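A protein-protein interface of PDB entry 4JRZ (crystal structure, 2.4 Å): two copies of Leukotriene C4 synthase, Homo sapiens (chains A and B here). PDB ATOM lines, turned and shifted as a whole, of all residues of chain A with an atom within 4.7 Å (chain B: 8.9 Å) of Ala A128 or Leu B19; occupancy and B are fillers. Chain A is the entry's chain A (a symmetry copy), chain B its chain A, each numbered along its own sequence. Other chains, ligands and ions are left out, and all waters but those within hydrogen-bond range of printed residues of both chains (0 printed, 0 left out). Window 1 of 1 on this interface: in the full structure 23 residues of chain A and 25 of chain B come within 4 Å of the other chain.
Among the printed residues, pairs that only touch across the chains: Thr A72 with Val B22, Ala A129 with Leu B19, Val A125 with Leu B23, Leu A132 with Ala B15, Leu A132 with Ala B16, Leu A132 with Leu B19, Leu A132 with Ala B12 and Ala A128 with Leu B19.
Of chain B, only Leu B19 comes within 4 Å of Ala A128. Leu B19 touches just these residues of chain A: Ala A128 (3.97 Å), Ala A129 (3.7 Å) and Leu A132 (3.95 Å). Of the printed residues of chain B, Thr A72 touches Val B22 (3.6 Å). Of the printed residues of chain A, Val B22 touches Thr A72 (3.6 Å). Phe B66 touches none of the printed residues of chain A. Gln B25 touches none of the printed residues of chain A. The nearest residue of chain B that does not touch Ala A128 is Ala B15 (6.8 Å).
Of the 22 printed residues of chain B, 6 touch a printed residue of chain A. Hydrophobic or aromatic side chains of chain B that line the printed part of chain A: Leu B19, Val B22 and Leu B23. Hydrophobic or aromatic side chains of chain A within 4 Å of the printed part of chain B: Val A125, Ala A128, Ala A129 and Leu A132.
No position is printed for both chains.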
ATOM      1  N   THR A  72     -17.159  32.709 -19.104  1.00  0.00           N
ATOM      2  CA  THR A  72     -17.793  31.965 -18.044  1.00  0.00           C
ATOM      3  C   THR A  72     -17.981  32.838 -16.818  1.00  0.00           C
ATOM      4  O   THR A  72     -18.879  32.609 -16.038  1.00  0.00           O
ATOM      5  CB  THR A  72     -16.939  30.746 -17.638  1.00  0.00           C
ATOM      6  OG1 THR A  72     -15.797  31.199 -16.905  1.00  0.00           O
ATOM      7  CG2 THR A  72     -16.466  30.005 -18.854  1.00  0.00           C
ATOM      8  N   VAL A  75     -21.312  34.770 -17.859  1.00  0.00           N
ATOM      9  CA  VAL A  75     -22.457  33.877 -17.780  1.00  0.00           C
ATOM     10  C   VAL A  75     -22.758  33.444 -16.354  1.00  0.00           C
ATOM     11  O   VAL A  75     -23.907  33.450 -15.933  1.00  0.00           O
ATOM     12  CB  VAL A  75     -22.285  32.643 -18.657  1.00  0.00           C
ATOM     13  CG1 VAL A  75     -23.521  31.752 -18.530  1.00  0.00           C
ATOM     14  CG2 VAL A  75     -22.036  33.081 -20.117  1.00  0.00           C
ATOM     15  N   ALA A  76     -21.731  33.079 -15.603  1.00  0.00           N
ATOM     16  CA  ALA A  76     -21.934  32.656 -14.227  1.00  0.00           C
ATOM     17  C   ALA A  76     -22.489  33.795 -13.376  1.00  0.00           C
ATOM     18  O   ALA A  76     -23.404  33.594 -12.600  1.00  0.00           O
ATOM     19  CB  ALA A  76     -20.625  32.126 -13.612  1.00  0.00           C
ATOM     20  N   LEU A 124     -16.479  28.232 -12.018  1.00  0.00           N
ATOM     21  CA  LEU A 124     -17.236  29.167 -12.853  1.00  0.00           C
ATOM     22  C   LEU A 124     -18.105  28.464 -13.894  1.00  0.00           C
ATOM     23  O   LEU A 124     -19.234  28.870 -14.132  1.00  0.00           O
ATOM     24  CB  LEU A 124     -16.310  30.176 -13.536  1.00  0.00           C
ATOM     25  CG  LEU A 124     -15.727  31.254 -12.632  1.00  0.00           C
ATOM     26  CD1 LEU A 124     -14.663  32.029 -13.377  1.00  0.00           C
ATOM     27  CD2 LEU A 124     -16.819  32.184 -12.128  1.00  0.00           C
ATOM     28  N   VAL A 125     -17.581  27.417 -14.517  1.00  0.00           N
ATOM     29  CA  VAL A 125     -18.329  26.695 -15.542  1.00  0.00           C
ATOM     30  C   VAL A 125     -19.521  25.981 -14.906  1.00  0.00           C
ATOM     31  O   VAL A 125     -20.593  25.853 -15.514  1.00  0.00           O
ATOM     32  CB  VAL A 125     -17.422  25.649 -16.278  1.00  0.00           C
ATOM     33  CG1 VAL A 125     -18.238  24.761 -17.215  1.00  0.00           C
ATOM     34  CG2 VAL A 125     -16.290  26.342 -17.050  1.00  0.00           C
ATOM     35  N   ALA A 126     -19.316  25.511 -13.677  1.00  0.00           N
ATOM     36  CA  ALA A 126     -20.320  24.741 -12.963  1.00  0.00           C
ATOM     37  C   ALA A 126     -21.479  25.668 -12.571  1.00  0.00           C
ATOM     38  O   ALA A 126     -22.657  25.369 -12.794  1.00  0.00           O
ATOM     39  CB  ALA A 126     -19.690  24.119 -11.726  1.00  0.00           C
ATOM     40  N   LEU A 127     -21.110  26.794 -11.980  1.00  0.00           N
ATOM     41  CA  LEU A 127     -22.038  27.865 -11.669  1.00  0.00           C
ATOM     42  C   LEU A 127     -22.813  28.312 -12.912  1.00  0.00           C
ATOM     43  O   LEU A 127     -24.041  28.353 -12.886  1.00  0.00           O
ATOM     44  CB  LEU A 127     -21.284  29.037 -11.054  1.00  0.00           C
ATOM     45  CG  LEU A 127     -20.657  28.730  -9.699  1.00  0.00           C
ATOM     46  CD1 LEU A 127     -20.194  30.013  -9.004  1.00  0.00           C
ATOM     47  CD2 LEU A 127     -21.646  27.950  -8.829  1.00  0.00           C
ATOM     48  N   ALA A 128     -22.102  28.617 -13.997  1.00  0.00           N
ATOM     49  CA  ALA A 128     -22.753  29.004 -15.249  1.00  0.00           C
ATOM     50  C   ALA A 128     -23.764  27.970 -15.697  1.00  0.00           C
ATOM     51  O   ALA A 128     -24.894  28.311 -16.025  1.00  0.00           O
ATOM     52  CB  ALA A 128     -21.728  29.238 -16.354  1.00  0.00           C
ATOM     53  N   ALA A 129     -23.351  26.707 -15.713  1.00  0.00           N
ATOM     54  CA  ALA A 129     -24.223  25.619 -16.157  1.00  0.00           C
ATOM     55  C   ALA A 129     -25.454  25.464 -15.267  1.00  0.00           C
ATOM     56  O   ALA A 129     -26.559  25.289 -15.766  1.00  0.00           O
ATOM     57  CB  ALA A 129     -23.456  24.307 -16.219  1.00  0.00           C
ATOM     58  N   LEU A 130     -25.249  25.515 -13.956  1.00  0.00           N
ATOM     59  CA  LEU A 130     -26.352  25.443 -13.005  1.00  0.00           C
ATOM     60  C   LEU A 130     -27.304  26.614 -13.225  1.00  0.00           C
ATOM     61  O   LEU A 130     -28.523  26.439 -13.264  1.00  0.00           O
ATOM     62  CB  LEU A 130     -25.824  25.458 -11.569  1.00  0.00           C
ATOM     63  CG  LEU A 130     -25.257  24.117 -11.102  1.00  0.00           C
ATOM     64  CD1 LEU A 130     -24.752  24.205  -9.665  1.00  0.00           C
ATOM     65  CD2 LEU A 130     -26.317  23.036 -11.247  1.00  0.00           C
ATOM     66  N   GLY A 131     -26.730  27.803 -13.387  1.00  0.00           N
ATOM     67  CA  GLY A 131     -27.499  29.003 -13.617  1.00  0.00           C
ATOM     68  C   GLY A 131     -28.356  28.902 -14.859  1.00  0.00           C
ATOM     69  O   GLY A 131     -29.486  29.368 -14.881  1.00  0.00           O
ATOM     70  N   LEU A 132     -27.821  28.292 -15.907  1.00  0.00           N
ATOM     71  CA  LEU A 132     -28.582  28.148 -17.139  1.00  0.00           C
ATOM     72  C   LEU A 132     -29.631  27.035 -17.037  1.00  0.00           C
ATOM     73  O   LEU A 132     -30.644  27.069 -17.727  1.00  0.00           O
ATOM     74  CB  LEU A 132     -27.641  27.899 -18.321  1.00  0.00           C
ATOM     75  CG  LEU A 132     -26.823  29.093 -18.837  1.00  0.00           C
ATOM     76  CD1 LEU A 132     -25.709  28.628 -19.802  1.00  0.00           C
ATOM     77  CD2 LEU A 132     -27.714  30.152 -19.505  1.00  0.00           C
ATOM     78  N   VAL B  11     -31.052  36.941 -23.643  1.00  0.00           N
ATOM     79  CA  VAL B  11     -29.700  36.532 -24.010  1.00  0.00           C
ATOM     80  C   VAL B  11     -29.311  35.113 -23.599  1.00  0.00           C
ATOM     81  O   VAL B  11     -28.149  34.754 -23.708  1.00  0.00           O
ATOM     82  CB  VAL B  11     -28.628  37.510 -23.455  1.00  0.00           C
ATOM     83  CG1 VAL B  11     -28.862  38.916 -23.957  1.00  0.00           C
ATOM     84  CG2 VAL B  11     -28.595  37.477 -21.949  1.00  0.00           C
ATOM     85  N   ALA B  12     -30.273  34.311 -23.152  1.00  0.00           N
ATOM     86  CA  ALA B  12     -29.962  33.036 -22.514  1.00  0.00           C
ATOM     87  C   ALA B  12     -29.552  31.988 -23.524  1.00  0.00           C
ATOM     88  O   ALA B  12     -28.808  31.079 -23.192  1.00  0.00           O
ATOM     89  CB  ALA B  12     -31.147  32.527 -21.684  1.00  0.00           C
ATOM     90  N   LEU B  13     -30.067  32.098 -24.741  1.00  0.00           N
ATOM     91  CA  LEU B  13     -29.680  31.180 -25.784  1.00  0.00           C
ATOM     92  C   LEU B  13     -28.233  31.507 -26.135  1.00  0.00           C
ATOM     93  O   LEU B  13     -27.434  30.603 -26.366  1.00  0.00           O
ATOM     94  CB  LEU B  13     -30.573  31.308 -27.034  1.00  0.00           C
ATOM     95  CG  LEU B  13     -32.046  30.903 -26.947  1.00  0.00           C
ATOM     96  CD1 LEU B  13     -32.771  31.116 -28.288  1.00  0.00           C
ATOM     97  CD2 LEU B  13     -32.232  29.477 -26.442  1.00  0.00           C
ATOM     98  N   LEU B  14     -27.906  32.799 -26.154  1.00  0.00           N
ATOM     99  CA  LEU B  14     -26.555  33.234 -26.489  1.00  0.00           C
ATOM    100  C   LEU B  14     -25.586  32.772 -25.412  1.00  0.00           C
ATOM    101  O   LEU B  14     -24.470  32.366 -25.711  1.00  0.00           O
ATOM    102  CB  LEU B  14     -26.484  34.755 -26.624  1.00  0.00           C
ATOM    103  CG  LEU B  14     -27.455  35.417 -27.606  1.00  0.00           C
ATOM    104  CD1 LEU B  14     -27.332  36.941 -27.550  1.00  0.00           C
ATOM    105  CD2 LEU B  14     -27.280  34.904 -29.017  1.00  0.00           C
ATOM    106  N   ALA B  15     -26.030  32.823 -24.158  1.00  0.00           N
ATOM    107  CA  ALA B  15     -25.185  32.424 -23.067  1.00  0.00           C
ATOM    108  C   ALA B  15     -25.002  30.906 -23.085  1.00  0.00           C
ATOM    109  O   ALA B  15     -23.958  30.387 -22.682  1.00  0.00           O
ATOM    110  CB  ALA B  15     -25.760  32.892 -21.745  1.00  0.00           C
ATOM    111  N   ALA B  16     -26.016  30.204 -23.569  1.00  0.00           N
ATOM    112  CA  ALA B  16     -25.978  28.752 -23.600  1.00  0.00           C
ATOM    113  C   ALA B  16     -24.978  28.281 -24.663  1.00  0.00           C
ATOM    114  O   ALA B  16     -24.177  27.384 -24.422  1.00  0.00           O
ATOM    115  CB  ALA B  16     -27.376  28.181 -23.872  1.00  0.00           C
ATOM    116  N   VAL B  17     -25.051  28.881 -25.846  1.00  0.00           N
ATOM    117  CA  VAL B  17     -24.095  28.601 -26.900  1.00  0.00           C
ATOM    118  C   VAL B  17     -22.659  29.002 -26.489  1.00  0.00           C
ATOM    119  O   VAL B  17     -21.708  28.282 -26.760  1.00  0.00           O
ATOM    120  CB  VAL B  17     -24.510  29.291 -28.176  1.00  0.00           C
ATOM    121  CG1 VAL B  17     -23.428  29.154 -29.258  1.00  0.00           C
ATOM    122  CG2 VAL B  17     -25.835  28.713 -28.649  1.00  0.00           C
ATOM    123  N   THR B  18     -22.529  30.133 -25.803  1.00  0.00           N
ATOM    124  CA  THR B  18     -21.256  30.613 -25.289  1.00  0.00           C
ATOM    125  C   THR B  18     -20.624  29.612 -24.314  1.00  0.00           C
ATOM    126  O   THR B  18     -19.416  29.364 -24.353  1.00  0.00           O
ATOM    127  CB  THR B  18     -21.458  31.966 -24.576  1.00  0.00           C
ATOM    128  OG1 THR B  18     -21.824  32.952 -25.541  1.00  0.00           O
ATOM    129  CG2 THR B  18     -20.202  32.413 -23.839  1.00  0.00           C
ATOM    130  N   LEU B  19     -21.438  29.043 -23.438  1.00  0.00           N
ATOM    131  CA  LEU B  19     -20.960  28.043 -22.490  1.00  0.00           C
ATOM    132  C   LEU B  19     -20.552  26.755 -23.209  1.00  0.00           C
ATOM    133  O   LEU B  19     -19.559  26.120 -22.855  1.00  0.00           O
ATOM    134  CB  LEU B  19     -22.021  27.730 -21.436  1.00  0.00           C
ATOM    135  CG  LEU B  19     -21.472  26.783 -20.362  1.00  0.00           C
ATOM    136  CD1 LEU B  19     -20.338  27.475 -19.624  1.00  0.00           C
ATOM    137  CD2 LEU B  19     -22.546  26.291 -19.399  1.00  0.00           C
ATOM    138  N   LEU B  20     -21.337  26.384 -24.214  1.00  0.00           N
ATOM    139  CA  LEU B  20     -21.043  25.240 -25.041  1.00  0.00           C
ATOM    140  C   LEU B  20     -19.683  25.447 -25.700  1.00  0.00           C
ATOM    141  O   LEU B  20     -18.861  24.532 -25.750  1.00  0.00           O
ATOM    142  CB  LEU B  20     -22.122  25.073 -26.110  1.00  0.00           C
ATOM    143  CG  LEU B  20     -21.926  23.879 -27.048  1.00  0.00           C
ATOM    144  CD1 LEU B  20     -21.878  22.546 -26.284  1.00  0.00           C
ATOM    145  CD2 LEU B  20     -23.002  23.853 -28.103  1.00  0.00           C
ATOM    146  N   GLY B  21     -19.458  26.666 -26.185  1.00  0.00           N
ATOM    147  CA  GLY B  21     -18.209  27.036 -26.824  1.00  0.00           C
ATOM    148  C   GLY B  21     -17.037  26.903 -25.872  1.00  0.00           C
ATOM    149  O   GLY B  21     -15.976  26.419 -26.250  1.00  0.00           O
ATOM    150  N   VAL B  22     -17.222  27.329 -24.629  1.00  0.00           N
ATOM    151  CA  VAL B  22     -16.154  27.211 -23.658  1.00  0.00           C
ATOM    152  C   VAL B  22     -15.804  25.744 -23.394  1.00  0.00           C
ATOM    153  O   VAL B  22     -14.631  25.371 -23.403  1.00  0.00           O
ATOM    154  CB  VAL B  22     -16.481  27.960 -22.353  1.00  0.00           C
ATOM    155  CG1 VAL B  22     -15.573  27.514 -21.231  1.00  0.00           C
ATOM    156  CG2 VAL B  22     -16.358  29.479 -22.579  1.00  0.00           C
ATOM    157  N   LEU B  23     -16.833  24.930 -23.178  1.00  0.00           N
ATOM    158  CA  LEU B  23     -16.692  23.497 -22.976  1.00  0.00           C
ATOM    159  C   LEU B  23     -15.985  22.828 -24.159  1.00  0.00           C
ATOM    160  O   LEU B  23     -15.218  21.896 -23.978  1.00  0.00           O
ATOM    161  CB  LEU B  23     -18.066  22.848 -22.756  1.00  0.00           C
ATOM    162  CG  LEU B  23     -18.726  23.068 -21.394  1.00  0.00           C
ATOM    163  CD1 LEU B  23     -20.043  22.294 -21.275  1.00  0.00           C
ATOM    164  CD2 LEU B  23     -17.780  22.673 -20.277  1.00  0.00           C
ATOM    165  N   LEU B  24     -16.239  23.311 -25.370  1.00  0.00           N
ATOM    166  CA  LEU B  24     -15.561  22.778 -26.536  1.00  0.00           C
ATOM    167  C   LEU B  24     -14.047  23.061 -26.476  1.00  0.00           C
ATOM    168  O   LEU B  24     -13.229  22.171 -26.715  1.00  0.00           O
ATOM    169  CB  LEU B  24     -16.181  23.337 -27.813  1.00  0.00           C
ATOM    170  CG  LEU B  24     -15.757  22.672 -29.126  1.00  0.00           C
ATOM    171  CD1 LEU B  24     -15.888  21.145 -29.040  1.00  0.00           C
ATOM    172  CD2 LEU B  24     -16.580  23.205 -30.285  1.00  0.00           C
ATOM    173  N   GLN B  25     -13.689  24.293 -26.123  1.00  0.00           N
ATOM    174  CA  GLN B  25     -12.298  24.703 -26.034  1.00  0.00           C
ATOM    175  C   GLN B  25     -11.549  23.969 -24.944  1.00  0.00           C
ATOM    176  O   GLN B  25     -10.347  23.742 -25.059  1.00  0.00           O
ATOM    177  CB  GLN B  25     -12.195  26.202 -25.770  1.00  0.00           C
ATOM    178  CG  GLN B  25     -12.826  27.029 -26.853  1.00  0.00           C
ATOM    179  CD  GLN B  25     -11.909  27.218 -28.026  1.00  0.00           C
ATOM    180  OE1 GLN B  25     -12.301  27.018 -29.167  1.00  0.00           O
ATOM    181  NE2 GLN B  25     -10.681  27.639 -27.756  1.00  0.00           N
ATOM    182  N   ALA B  26     -12.244  23.626 -23.871  1.00  0.00           N
ATOM    183  CA  ALA B  26     -11.586  22.935 -22.786  1.00  0.00           C
ATOM    184  C   ALA B  26     -11.342  21.502 -23.241  1.00  0.00           C
ATOM    185  O   ALA B  26     -10.324  20.897 -22.906  1.00  0.00           O
ATOM    186  CB  ALA B  26     -12.420  22.988 -21.510  1.00  0.00           C
ATOM    187  N   PHE B  66     -12.164  31.908 -31.431  1.00  0.00           N
ATOM    188  CA  PHE B  66     -13.196  31.858 -30.415  1.00  0.00           C
ATOM    189  C   PHE B  66     -13.730  33.249 -29.960  1.00  0.00           C
ATOM    190  O   PHE B  66     -14.934  33.417 -29.872  1.00  0.00           O
ATOM    191  CB  PHE B  66     -12.730  31.009 -29.234  1.00  0.00           C
ATOM    192  CG  PHE B  66     -13.781  30.792 -28.193  1.00  0.00           C
ATOM    193  CD1 PHE B  66     -14.906  30.038 -28.474  1.00  0.00           C
ATOM    194  CD2 PHE B  66     -13.637  31.326 -26.925  1.00  0.00           C
ATOM    195  CE1 PHE B  66     -15.889  29.826 -27.506  1.00  0.00           C
ATOM    196  CE2 PHE B  66     -14.614  31.114 -25.950  1.00  0.00           C
ATOM    197  CZ  PHE B  66     -15.730  30.366 -26.242  1.00  0.00           C
ATOM    198  N   PHE B  69     -15.869  34.619 -32.767  1.00  0.00           N
ATOM    199  CA  PHE B  69     -17.130  33.945 -32.724  1.00  0.00           C
ATOM    200  C   PHE B  69     -18.044  34.531 -31.634  1.00  0.00           C
ATOM    201  O   PHE B  69     -19.187  34.848 -31.898  1.00  0.00           O
ATOM    202  CB  PHE B  69     -16.886  32.474 -32.457  1.00  0.00           C
ATOM    203  CG  PHE B  69     -18.108  31.731 -32.042  1.00  0.00           C
ATOM    204  CD1 PHE B  69     -19.195  31.645 -32.879  1.00  0.00           C
ATOM    205  CD2 PHE B  69     -18.156  31.094 -30.828  1.00  0.00           C
ATOM    206  CE1 PHE B  69     -20.310  30.945 -32.497  1.00  0.00           C
ATOM    207  CE2 PHE B  69     -19.277  30.394 -30.449  1.00  0.00           C
ATOM    208  CZ  PHE B  69     -20.343  30.328 -31.283  1.00  0.00           C
ATOM    209  N   LEU B  70     -17.520  34.642 -30.417  1.00  0.00           N
ATOM    210  CA  LEU B  70     -18.231  35.205 -29.293  1.00  0.00           C
ATOM    211  C   LEU B  70     -18.743  36.627 -29.588  1.00  0.00           C
ATOM    212  O   LEU B  70     -19.908  36.951 -29.322  1.00  0.00           O
ATOM    213  CB  LEU B  70     -17.314  35.240 -28.063  1.00  0.00           C
ATOM    214  CG  LEU B  70     -16.972  33.913 -27.388  1.00  0.00           C
ATOM    215  CD1 LEU B  70     -16.203  34.178 -26.125  1.00  0.00           C
ATOM    216  CD2 LEU B  70     -18.225  33.071 -27.092  1.00  0.00           C
ATOM    217  N   LEU B  73     -21.480  36.563 -32.316  1.00  0.00           N
ATOM    218  CA  LEU B  73     -22.629  35.866 -31.785  1.00  0.00           C
ATOM    219  C   LEU B  73     -23.485  36.855 -30.941  1.00  0.00           C
ATOM    220  O   LEU B  73     -24.696  36.917 -31.085  1.00  0.00           O
ATOM    221  CB  LEU B  73     -22.182  34.666 -30.935  1.00  0.00           C
ATOM    222  CG  LEU B  73     -23.299  33.908 -30.182  1.00  0.00           C
ATOM    223  CD1 LEU B  73     -24.180  33.103 -31.120  1.00  0.00           C
ATOM    224  CD2 LEU B  73     -22.754  33.022 -29.059  1.00  0.00           C
ATOM    225  N   TRP B  74     -22.836  37.624 -30.074  1.00  0.00           N
ATOM    226  CA  TRP B  74     -23.524  38.549 -29.175  1.00  0.00           C
ATOM    227  C   TRP B  74     -24.091  39.776 -29.872  1.00  0.00           C
ATOM    228  O   TRP B  74     -25.215  40.170 -29.588  1.00  0.00           O
ATOM    229  CB  TRP B  74     -22.645  38.932 -27.983  1.00  0.00           C
ATOM    230  CG  TRP B  74     -22.669  37.825 -26.972  1.00  0.00           C
ATOM    231  CD1 TRP B  74     -21.892  36.715 -26.966  1.00  0.00           C
ATOM    232  CD2 TRP B  74     -23.566  37.693 -25.865  1.00  0.00           C
ATOM    233  NE1 TRP B  74     -22.233  35.898 -25.919  1.00  0.00           N
ATOM    234  CE2 TRP B  74     -23.254  36.479 -25.220  1.00  0.00           C
ATOM    235  CE3 TRP B  74     -24.584  38.496 -25.342  1.00  0.00           C
ATOM    236  CZ2 TRP B  74     -23.924  36.045 -24.071  1.00  0.00           C
ATOM    237  CZ3 TRP B  74     -25.254  38.061 -24.214  1.00  0.00           C
ATOM    238  CH2 TRP B  74     -24.926  36.846 -23.593  1.00  0.00           C
ATOM    239  N   LEU B  93     -19.984  25.735 -33.880  1.00  0.00           N
ATOM    240  CA  LEU B  93     -19.264  24.958 -32.887  1.00  0.00           C
ATOM    241  C   LEU B  93     -19.172  23.481 -33.271  1.00  0.00           C
ATOM    242  O   LEU B  93     -18.223  22.778 -32.909  1.00  0.00           O
ATOM    243  CB  LEU B  93     -19.955  25.095 -31.528  1.00  0.00           C
ATOM    244  CG  LEU B  93     -19.857  26.487 -30.905  1.00  0.00           C
ATOM    245  CD1 LEU B  93     -20.728  26.550 -29.647  1.00  0.00           C
ATOM    246  CD2 LEU B  93     -18.373  26.839 -30.602  1.00  0.00           C
